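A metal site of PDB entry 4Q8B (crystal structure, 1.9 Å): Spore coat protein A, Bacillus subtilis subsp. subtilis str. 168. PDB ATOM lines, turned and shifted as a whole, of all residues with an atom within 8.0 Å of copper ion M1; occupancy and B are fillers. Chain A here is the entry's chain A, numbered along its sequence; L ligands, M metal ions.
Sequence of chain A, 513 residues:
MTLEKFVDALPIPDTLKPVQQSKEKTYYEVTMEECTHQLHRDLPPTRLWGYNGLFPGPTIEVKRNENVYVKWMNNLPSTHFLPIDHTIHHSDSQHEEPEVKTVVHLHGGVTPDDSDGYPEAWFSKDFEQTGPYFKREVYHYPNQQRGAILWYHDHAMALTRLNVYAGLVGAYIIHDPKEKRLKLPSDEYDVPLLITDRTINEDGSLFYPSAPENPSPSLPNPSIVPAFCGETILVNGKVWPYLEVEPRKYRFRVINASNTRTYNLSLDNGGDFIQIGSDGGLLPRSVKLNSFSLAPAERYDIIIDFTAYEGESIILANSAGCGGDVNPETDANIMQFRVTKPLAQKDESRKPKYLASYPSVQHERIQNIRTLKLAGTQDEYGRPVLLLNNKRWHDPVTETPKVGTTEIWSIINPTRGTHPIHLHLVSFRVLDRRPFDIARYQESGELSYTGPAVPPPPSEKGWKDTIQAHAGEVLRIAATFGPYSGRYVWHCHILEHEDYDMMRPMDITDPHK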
ATOM      1  N   HIS A 105      22.298   0.891   9.207  1.00  0.00           N
ATOM      2  CA  HIS A 105      22.640   2.289   9.083  1.00  0.00           C
ATOM      3  C   HIS A 105      22.916   2.834  10.452  1.00  0.00           C
ATOM      4  O   HIS A 105      22.083   2.711  11.342  1.00  0.00           O
ATOM      5  CB  HIS A 105      21.483   3.045   8.449  1.00  0.00           C
ATOM      6  CG  HIS A 105      21.649   4.538   8.411  1.00  0.00           C
ATOM      7  ND1 HIS A 105      22.720   5.166   7.804  1.00  0.00           N
ATOM      8  CD2 HIS A 105      20.881   5.522   8.928  1.00  0.00           C
ATOM      9  CE1 HIS A 105      22.598   6.475   7.938  1.00  0.00           C
ATOM     10  NE2 HIS A 105      21.477   6.706   8.616  1.00  0.00           N
ATOM     11  N   LEU A 106      24.056   3.488  10.580  1.00  0.00           N
ATOM     12  CA  LEU A 106      24.396   4.314  11.705  1.00  0.00           C
ATOM     13  C   LEU A 106      23.826   5.726  11.494  1.00  0.00           C
ATOM     14  O   LEU A 106      24.401   6.530  10.741  1.00  0.00           O
ATOM     15  CB  LEU A 106      25.928   4.356  11.933  1.00  0.00           C
ATOM     16  CG  LEU A 106      26.411   5.210  13.101  1.00  0.00           C
ATOM     17  CD1 LEU A 106      25.783   4.756  14.420  1.00  0.00           C
ATOM     18  CD2 LEU A 106      27.922   5.171  13.250  1.00  0.00           C
ATOM     19  N   HIS A 107      22.709   6.003  12.152  1.00  0.00           N
ATOM     20  CA  HIS A 107      21.967   7.223  11.963  1.00  0.00           C
ATOM     21  C   HIS A 107      22.714   8.326  12.623  1.00  0.00           C
ATOM     22  O   HIS A 107      22.970   8.290  13.824  1.00  0.00           O
ATOM     23  CB  HIS A 107      20.546   7.120  12.526  1.00  0.00           C
ATOM     24  CG  HIS A 107      19.710   8.310  12.296  1.00  0.00           C
ATOM     25  ND1 HIS A 107      18.509   8.267  11.621  1.00  0.00           N
ATOM     26  CD2 HIS A 107      19.922   9.618  12.588  1.00  0.00           C
ATOM     27  CE1 HIS A 107      18.005   9.479  11.534  1.00  0.00           C
ATOM     28  NE2 HIS A 107      18.856  10.310  12.098  1.00  0.00           N
ATOM     29  N   GLY A 108      23.049   9.304  11.814  1.00  0.00           N
ATOM     30  CA  GLY A 108      23.962  10.387  12.221  1.00  0.00           C
ATOM     31  C   GLY A 108      25.445  10.170  11.951  1.00  0.00           C
ATOM     32  O   GLY A 108      26.233  11.050  12.174  1.00  0.00           O
ATOM     33  N   TRP A 151      22.303   6.530  16.641  1.00  0.00           N
ATOM     34  CA  TRP A 151      21.675   5.262  16.883  1.00  0.00           C
ATOM     35  C   TRP A 151      21.760   4.463  15.608  1.00  0.00           C
ATOM     36  O   TRP A 151      22.016   5.016  14.530  1.00  0.00           O
ATOM     37  CB  TRP A 151      20.215   5.430  17.358  1.00  0.00           C
ATOM     38  CG  TRP A 151      19.212   6.063  16.459  1.00  0.00           C
ATOM     39  CD1 TRP A 151      19.267   7.307  15.921  1.00  0.00           C
ATOM     40  CD2 TRP A 151      17.997   5.480  15.974  1.00  0.00           C
ATOM     41  NE1 TRP A 151      18.178   7.540  15.167  1.00  0.00           N
ATOM     42  CE2 TRP A 151      17.369   6.431  15.179  1.00  0.00           C
ATOM     43  CE3 TRP A 151      17.373   4.231  16.127  1.00  0.00           C
ATOM     44  CZ2 TRP A 151      16.155   6.199  14.555  1.00  0.00           C
ATOM     45  CZ3 TRP A 151      16.189   4.004  15.506  1.00  0.00           C
ATOM     46  CH2 TRP A 151      15.585   4.987  14.729  1.00  0.00           C
ATOM     47  N   TYR A 152      21.666   3.159  15.752  1.00  0.00           N
ATOM     48  CA  TYR A 152      21.779   2.259  14.590  1.00  0.00           C
ATOM     49  C   TYR A 152      20.504   1.449  14.442  1.00  0.00           C
ATOM     50  O   TYR A 152      19.865   1.093  15.433  1.00  0.00           O
ATOM     51  CB  TYR A 152      23.012   1.414  14.716  1.00  0.00           C
ATOM     52  CG  TYR A 152      23.114   0.439  15.902  1.00  0.00           C
ATOM     53  CD1 TYR A 152      22.775  -0.915  15.769  1.00  0.00           C
ATOM     54  CD2 TYR A 152      23.535   0.851  17.146  1.00  0.00           C
ATOM     55  CE1 TYR A 152      22.851  -1.797  16.831  1.00  0.00           C
ATOM     56  CE2 TYR A 152      23.634  -0.049  18.215  1.00  0.00           C
ATOM     57  CZ  TYR A 152      23.272  -1.369  18.047  1.00  0.00           C
ATOM     58  OH  TYR A 152      23.358  -2.263  19.128  1.00  0.00           O
ATOM     59  N   HIS A 153      20.137   1.142  13.193  1.00  0.00           N
ATOM     60  CA  HIS A 153      18.898   0.481  12.915  1.00  0.00           C
ATOM     61  C   HIS A 153      18.913  -0.089  11.523  1.00  0.00           C
ATOM     62  O   HIS A 153      19.703   0.349  10.627  1.00  0.00           O
ATOM     63  CB  HIS A 153      17.704   1.436  13.090  1.00  0.00           C
ATOM     64  CG  HIS A 153      17.673   2.635  12.191  1.00  0.00           C
ATOM     65  ND1 HIS A 153      17.248   2.576  10.891  1.00  0.00           N
ATOM     66  CD2 HIS A 153      17.940   3.942  12.434  1.00  0.00           C
ATOM     67  CE1 HIS A 153      17.312   3.774  10.333  1.00  0.00           C
ATOM     68  NE2 HIS A 153      17.661   4.629  11.280  1.00  0.00           N
ATOM     69  N   ASP A 154      18.013  -1.029  11.291  1.00  0.00           N
ATOM     70  CA  ASP A 154      17.884  -1.616   9.951  1.00  0.00           C
ATOM     71  C   ASP A 154      17.404  -0.586   8.913  1.00  0.00           C
ATOM     72  O   ASP A 154      16.717   0.371   9.234  1.00  0.00           O
ATOM     73  CB  ASP A 154      16.961  -2.808   9.909  1.00  0.00           C
ATOM     74  CG  ASP A 154      17.069  -3.541   8.588  1.00  0.00           C
ATOM     75  OD1 ASP A 154      16.239  -3.272   7.700  1.00  0.00           O
ATOM     76  OD2 ASP A 154      18.054  -4.305   8.455  1.00  0.00           O
ATOM     77  N   HIS A 155      17.875  -0.740   7.682  1.00  0.00           N
ATOM     78  CA  HIS A 155      17.541   0.215   6.635  1.00  0.00           C
ATOM     79  C   HIS A 155      17.287  -0.483   5.316  1.00  0.00           C
ATOM     80  O   HIS A 155      17.399   0.119   4.273  1.00  0.00           O
ATOM     81  CB  HIS A 155      18.704   1.222   6.482  1.00  0.00           C
ATOM     82  CG  HIS A 155      18.297   2.615   6.059  1.00  0.00           C
ATOM     83  ND1 HIS A 155      17.613   2.876   4.889  1.00  0.00           N
ATOM     84  CD2 HIS A 155      18.524   3.827   6.628  1.00  0.00           C
ATOM     85  CE1 HIS A 155      17.440   4.188   4.765  1.00  0.00           C
ATOM     86  NE2 HIS A 155      17.990   4.782   5.798  1.00  0.00           N
ATOM     87  N   THR A 160      12.156  -1.523   5.906  1.00  0.00           N
ATOM     88  CA  THR A 160      12.634  -0.814   7.073  1.00  0.00           C
ATOM     89  C   THR A 160      11.603  -0.723   8.205  1.00  0.00           C
ATOM     90  O   THR A 160      11.929  -0.934   9.413  1.00  0.00           O
ATOM     91  CB  THR A 160      13.167   0.574   6.617  1.00  0.00           C
ATOM     92  OG1 THR A 160      14.312   0.342   5.766  1.00  0.00           O
ATOM     93  CG2 THR A 160      13.602   1.387   7.846  1.00  0.00           C
ATOM     94  N   VAL A 164      12.685  -2.599  11.655  1.00  0.00           N
ATOM     95  CA  VAL A 164      12.816  -1.777  12.863  1.00  0.00           C
ATOM     96  C   VAL A 164      11.778  -2.165  13.943  1.00  0.00           C
ATOM     97  O   VAL A 164      12.085  -2.313  15.132  1.00  0.00           O
ATOM     98  CB  VAL A 164      12.727  -0.300  12.471  1.00  0.00           C
ATOM     99  CG1 VAL A 164      12.708   0.613  13.702  1.00  0.00           C
ATOM    100  CG2 VAL A 164      13.910   0.043  11.583  1.00  0.00           C
ATOM    101  N   ASN A 256      13.906   8.785  19.769  1.00  0.00           N
ATOM    102  CA  ASN A 256      12.639   8.283  19.248  1.00  0.00           C
ATOM    103  C   ASN A 256      12.873   7.235  18.161  1.00  0.00           C
ATOM    104  O   ASN A 256      13.189   7.581  17.030  1.00  0.00           O
ATOM    105  CB  ASN A 256      11.740   9.388  18.721  1.00  0.00           C
ATOM    106  CG  ASN A 256      10.395   8.866  18.325  1.00  0.00           C
ATOM    107  OD1 ASN A 256      10.196   7.639  18.205  1.00  0.00           O
ATOM    108  ND2 ASN A 256       9.444   9.771  18.111  1.00  0.00           N
ATOM    109  N   PRO A 296      10.005  10.790  15.017  1.00  0.00           N
ATOM    110  CA  PRO A 296      10.858   9.681  14.722  1.00  0.00           C
ATOM    111  C   PRO A 296      12.282  10.052  14.320  1.00  0.00           C
ATOM    112  O   PRO A 296      12.498  10.956  13.511  1.00  0.00           O
ATOM    113  CB  PRO A 296      10.107   8.946  13.589  1.00  0.00           C
ATOM    114  CG  PRO A 296       8.688   9.204  13.871  1.00  0.00           C
ATOM    115  CD  PRO A 296       8.689  10.640  14.355  1.00  0.00           C
ATOM    116  N   ALA A 297      13.255   9.411  14.981  1.00  0.00           N
ATOM    117  CA  ALA A 297      14.704   9.599  14.777  1.00  0.00           C
ATOM    118  C   ALA A 297      15.340  10.837  15.389  1.00  0.00           C
ATOM    119  O   ALA A 297      16.563  10.977  15.318  1.00  0.00           O
ATOM    120  CB  ALA A 297      15.115   9.482  13.315  1.00  0.00           C
ATOM    121  N   GLU A 298      14.551  11.730  15.978  1.00  0.00           N
ATOM    122  CA  GLU A 298      15.140  12.872  16.609  1.00  0.00           C
ATOM    123  C   GLU A 298      15.749  12.390  17.923  1.00  0.00           C
ATOM    124  O   GLU A 298      15.268  11.410  18.510  1.00  0.00           O
ATOM    125  CB  GLU A 298      14.129  13.985  16.837  1.00  0.00           C
ATOM    126  CG  GLU A 298      13.606  14.658  15.577  1.00  0.00           C
ATOM    127  CD  GLU A 298      12.821  15.933  15.932  1.00  0.00           C
ATOM    128  OE1 GLU A 298      11.651  15.821  16.421  1.00  0.00           O
ATOM    129  OE2 GLU A 298      13.406  17.053  15.769  1.00  0.00           O
ATOM    130  N   ARG A 299      16.809  13.070  18.351  1.00  0.00           N
ATOM    131  CA  ARG A 299      17.471  12.837  19.619  1.00  0.00           C
ATOM    132  C   ARG A 299      17.524  14.125  20.412  1.00  0.00           C
ATOM    133  O   ARG A 299      17.741  15.210  19.836  1.00  0.00           O
ATOM    134  CB  ARG A 299      18.888  12.290  19.480  1.00  0.00           C
ATOM    135  CG  ARG A 299      18.882  10.832  19.093  1.00  0.00           C
ATOM    136  CD  ARG A 299      18.860  10.703  17.600  1.00  0.00           C
ATOM    137  NE  ARG A 299      20.167  11.116  17.038  1.00  0.00           N
ATOM    138  CZ  ARG A 299      20.349  11.628  15.836  1.00  0.00           C
ATOM    139  NH1 ARG A 299      19.324  11.813  15.023  1.00  0.00           N
ATOM    140  NH2 ARG A 299      21.574  11.973  15.431  1.00  0.00           N
ATOM    141  N   HIS A 422      15.119  13.586   7.168  1.00  0.00           N
ATOM    142  CA  HIS A 422      16.482  13.187   7.518  1.00  0.00           C
ATOM    143  C   HIS A 422      17.370  13.153   6.280  1.00  0.00           C
ATOM    144  O   HIS A 422      17.008  12.595   5.242  1.00  0.00           O
ATOM    145  CB  HIS A 422      16.458  11.816   8.194  1.00  0.00           C
ATOM    146  CG  HIS A 422      17.801  11.252   8.519  1.00  0.00           C
ATOM    147  ND1 HIS A 422      18.781  11.927   9.198  1.00  0.00           N
ATOM    148  CD2 HIS A 422      18.318  10.015   8.243  1.00  0.00           C
ATOM    149  CE1 HIS A 422      19.838  11.150   9.342  1.00  0.00           C
ATOM    150  NE2 HIS A 422      19.573   9.981   8.781  1.00  0.00           N
ATOM    151  N   HIS A 424      21.126  11.838   5.245  1.00  0.00           N
ATOM    152  CA  HIS A 424      22.321  11.129   5.686  1.00  0.00           C
ATOM    153  C   HIS A 424      23.558  11.971   5.593  1.00  0.00           C
ATOM    154  O   HIS A 424      23.519  13.074   5.000  1.00  0.00           O
ATOM    155  CB  HIS A 424      22.550   9.867   4.870  1.00  0.00           C
ATOM    156  CG  HIS A 424      21.549   8.803   5.140  1.00  0.00           C
ATOM    157  ND1 HIS A 424      21.864   7.460   5.088  1.00  0.00           N
ATOM    158  CD2 HIS A 424      20.246   8.879   5.500  1.00  0.00           C
ATOM    159  CE1 HIS A 424      20.765   6.748   5.328  1.00  0.00           C
ATOM    160  NE2 HIS A 424      19.785   7.584   5.620  1.00  0.00           N
ATOM    161  N   ASP A 465      19.925  16.558  12.275  1.00  0.00           N
ATOM    162  CA  ASP A 465      19.973  15.688  11.106  1.00  0.00           C
ATOM    163  C   ASP A 465      18.589  15.207  10.728  1.00  0.00           C
ATOM    164  O   ASP A 465      18.378  14.691   9.625  1.00  0.00           O
ATOM    165  CB  ASP A 465      21.035  14.596  11.223  1.00  0.00           C
ATOM    166  CG  ASP A 465      20.744  13.544  12.273  1.00  0.00           C
ATOM    167  OD1 ASP A 465      19.584  13.122  12.409  1.00  0.00           O
ATOM    168  OD2 ASP A 465      21.729  13.170  12.962  1.00  0.00           O
ATOM    169  N   THR A 466      17.622  15.390  11.627  1.00  0.00           N
ATOM    170  CA  THR A 466      16.256  14.977  11.387  1.00  0.00           C
ATOM    171  C   THR A 466      15.389  16.156  11.830  1.00  0.00           C
ATOM    172  O   THR A 466      15.565  16.629  12.954  1.00  0.00           O
ATOM    173  CB  THR A 466      15.919  13.678  12.137  1.00  0.00           C
ATOM    174  OG1 THR A 466      16.842  12.626  11.734  1.00  0.00           O
ATOM    175  CG2 THR A 466      14.528  13.263  11.834  1.00  0.00           C
ATOM    176  N   HIS A 491      15.342  11.267   3.194  1.00  0.00           N
ATOM    177  CA  HIS A 491      14.026  10.711   3.284  1.00  0.00           C
ATOM    178  C   HIS A 491      13.270  11.227   4.520  1.00  0.00           C
ATOM    179  O   HIS A 491      13.870  11.810   5.450  1.00  0.00           O
ATOM    180  CB  HIS A 491      14.059   9.165   3.361  1.00  0.00           C
ATOM    181  CG  HIS A 491      14.919   8.620   4.458  1.00  0.00           C
ATOM    182  ND1 HIS A 491      14.424   8.258   5.700  1.00  0.00           N
ATOM    183  CD2 HIS A 491      16.244   8.350   4.497  1.00  0.00           C
ATOM    184  CE1 HIS A 491      15.407   7.808   6.454  1.00  0.00           C
ATOM    185  NE2 HIS A 491      16.515   7.849   5.752  1.00  0.00           N
ATOM    186  N   HIS A 493      11.489  10.198   7.867  1.00  0.00           N
ATOM    187  CA  HIS A 493      11.798   9.129   8.837  1.00  0.00           C
ATOM    188  C   HIS A 493      10.591   8.540   9.539  1.00  0.00           C
ATOM    189  O   HIS A 493      10.768   7.728  10.456  1.00  0.00           O
ATOM    190  CB  HIS A 493      12.843   9.573   9.838  1.00  0.00           C
ATOM    191  CG  HIS A 493      13.778   8.487  10.258  1.00  0.00           C
ATOM    192  ND1 HIS A 493      13.347   7.395  10.976  1.00  0.00           N
ATOM    193  CD2 HIS A 493      15.096   8.307  10.060  1.00  0.00           C
ATOM    194  CE1 HIS A 493      14.361   6.592  11.205  1.00  0.00           C
ATOM    195  NE2 HIS A 493      15.440   7.131  10.681  1.00  0.00           N
ATOM    196  N   LEU A 495       8.559   5.631   9.069  1.00  0.00           N
ATOM    197  CA  LEU A 495       9.047   4.518   8.266  1.00  0.00           C
ATOM    198  C   LEU A 495       8.028   4.037   7.268  1.00  0.00           C
ATOM    199  O   LEU A 495       8.387   3.525   6.159  1.00  0.00           O
ATOM    200  CB  LEU A 495       9.541   3.359   9.142  1.00  0.00           C
ATOM    201  CG  LEU A 495      10.633   3.775  10.119  1.00  0.00           C
ATOM    202  CD1 LEU A 495      11.079   2.564  10.951  1.00  0.00           C
ATOM    203  CD2 LEU A 495      11.818   4.367   9.437  1.00  0.00           C
ATOM    204  N   GLU A 498       8.739   6.479   4.355  1.00  0.00           N
ATOM    205  CA  GLU A 498      10.035   6.054   3.817  1.00  0.00           C
ATOM    206  C   GLU A 498       9.895   4.879   2.851  1.00  0.00           C
ATOM    207  O   GLU A 498      10.473   4.924   1.759  1.00  0.00           O
ATOM    208  CB  GLU A 498      10.974   5.680   4.964  1.00  0.00           C
ATOM    209  CG  GLU A 498      12.403   5.384   4.521  1.00  0.00           C
ATOM    210  CD  GLU A 498      13.322   5.054   5.687  1.00  0.00           C
ATOM    211  OE1 GLU A 498      13.122   5.581   6.817  1.00  0.00           O
ATOM    212  OE2 GLU A 498      14.278   4.278   5.438  1.00  0.00           O
HETATM  213  O1  LIG L   1      17.453   6.219   8.440  1.00  0.00           O
HETATM  214  O2  LIG L   1      18.146   7.204   8.621  1.00  0.00           O
HETATM  215 CU    CU M   1      17.510   6.566  11.067  1.00  0.00          CU
HETATM  216 CU    CU M   2      20.416   8.295   8.709  1.00  0.00          CU
HETATM  217 CU    CU M   3      18.053   6.764   6.259  1.00  0.00          CU
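The backbone carbonyl oxygen (O) of His 153 is in hydrogen-bond range of the backbone NH (N) of His 105, 3.0 Å away.
The backbone carbonyl oxygen of Trp 151 sits at hydrogen-bond distance from the backbone NH of His 107 (2.7 Å).
A ring nitrogen (NE2) of His 107 lies close to a ring nitrogen (ND1) of His 422 (3.3 Å).
The side-chain hydroxyl of Thr 466 lies within hydrogen-bond range of a ring nitrogen (NE2) of His 107.
A ring nitrogen (NE2) of His 107 is in hydrogen-bond range of the guanidinium group of Arg 299, at 3.3 Å.
A ring nitrogen (NE2) of His 107 is in hydrogen-bond range of the side-chain carboxylate (OD1) of Asp 465 (2.9 Å).
Copper ion M1 is bound by a ring nitrogen (NE2) of His 153 (2.0 Å), a ring nitrogen (ND1) of His 107 (2.0 Å) and a ring nitrogen (NE2) of His 493 (2.2 Å).
Slightly farther from copper ion M1 lies O2 of the ligand (2.6 Å).
Merely in contact with copper ion M1: Trp 151.
Of the 24 residues printed, 4 come within 4 Å of copper ion M1.
Along chain A the residues within 4 Å of copper ion M1 span positions 107 to 493.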
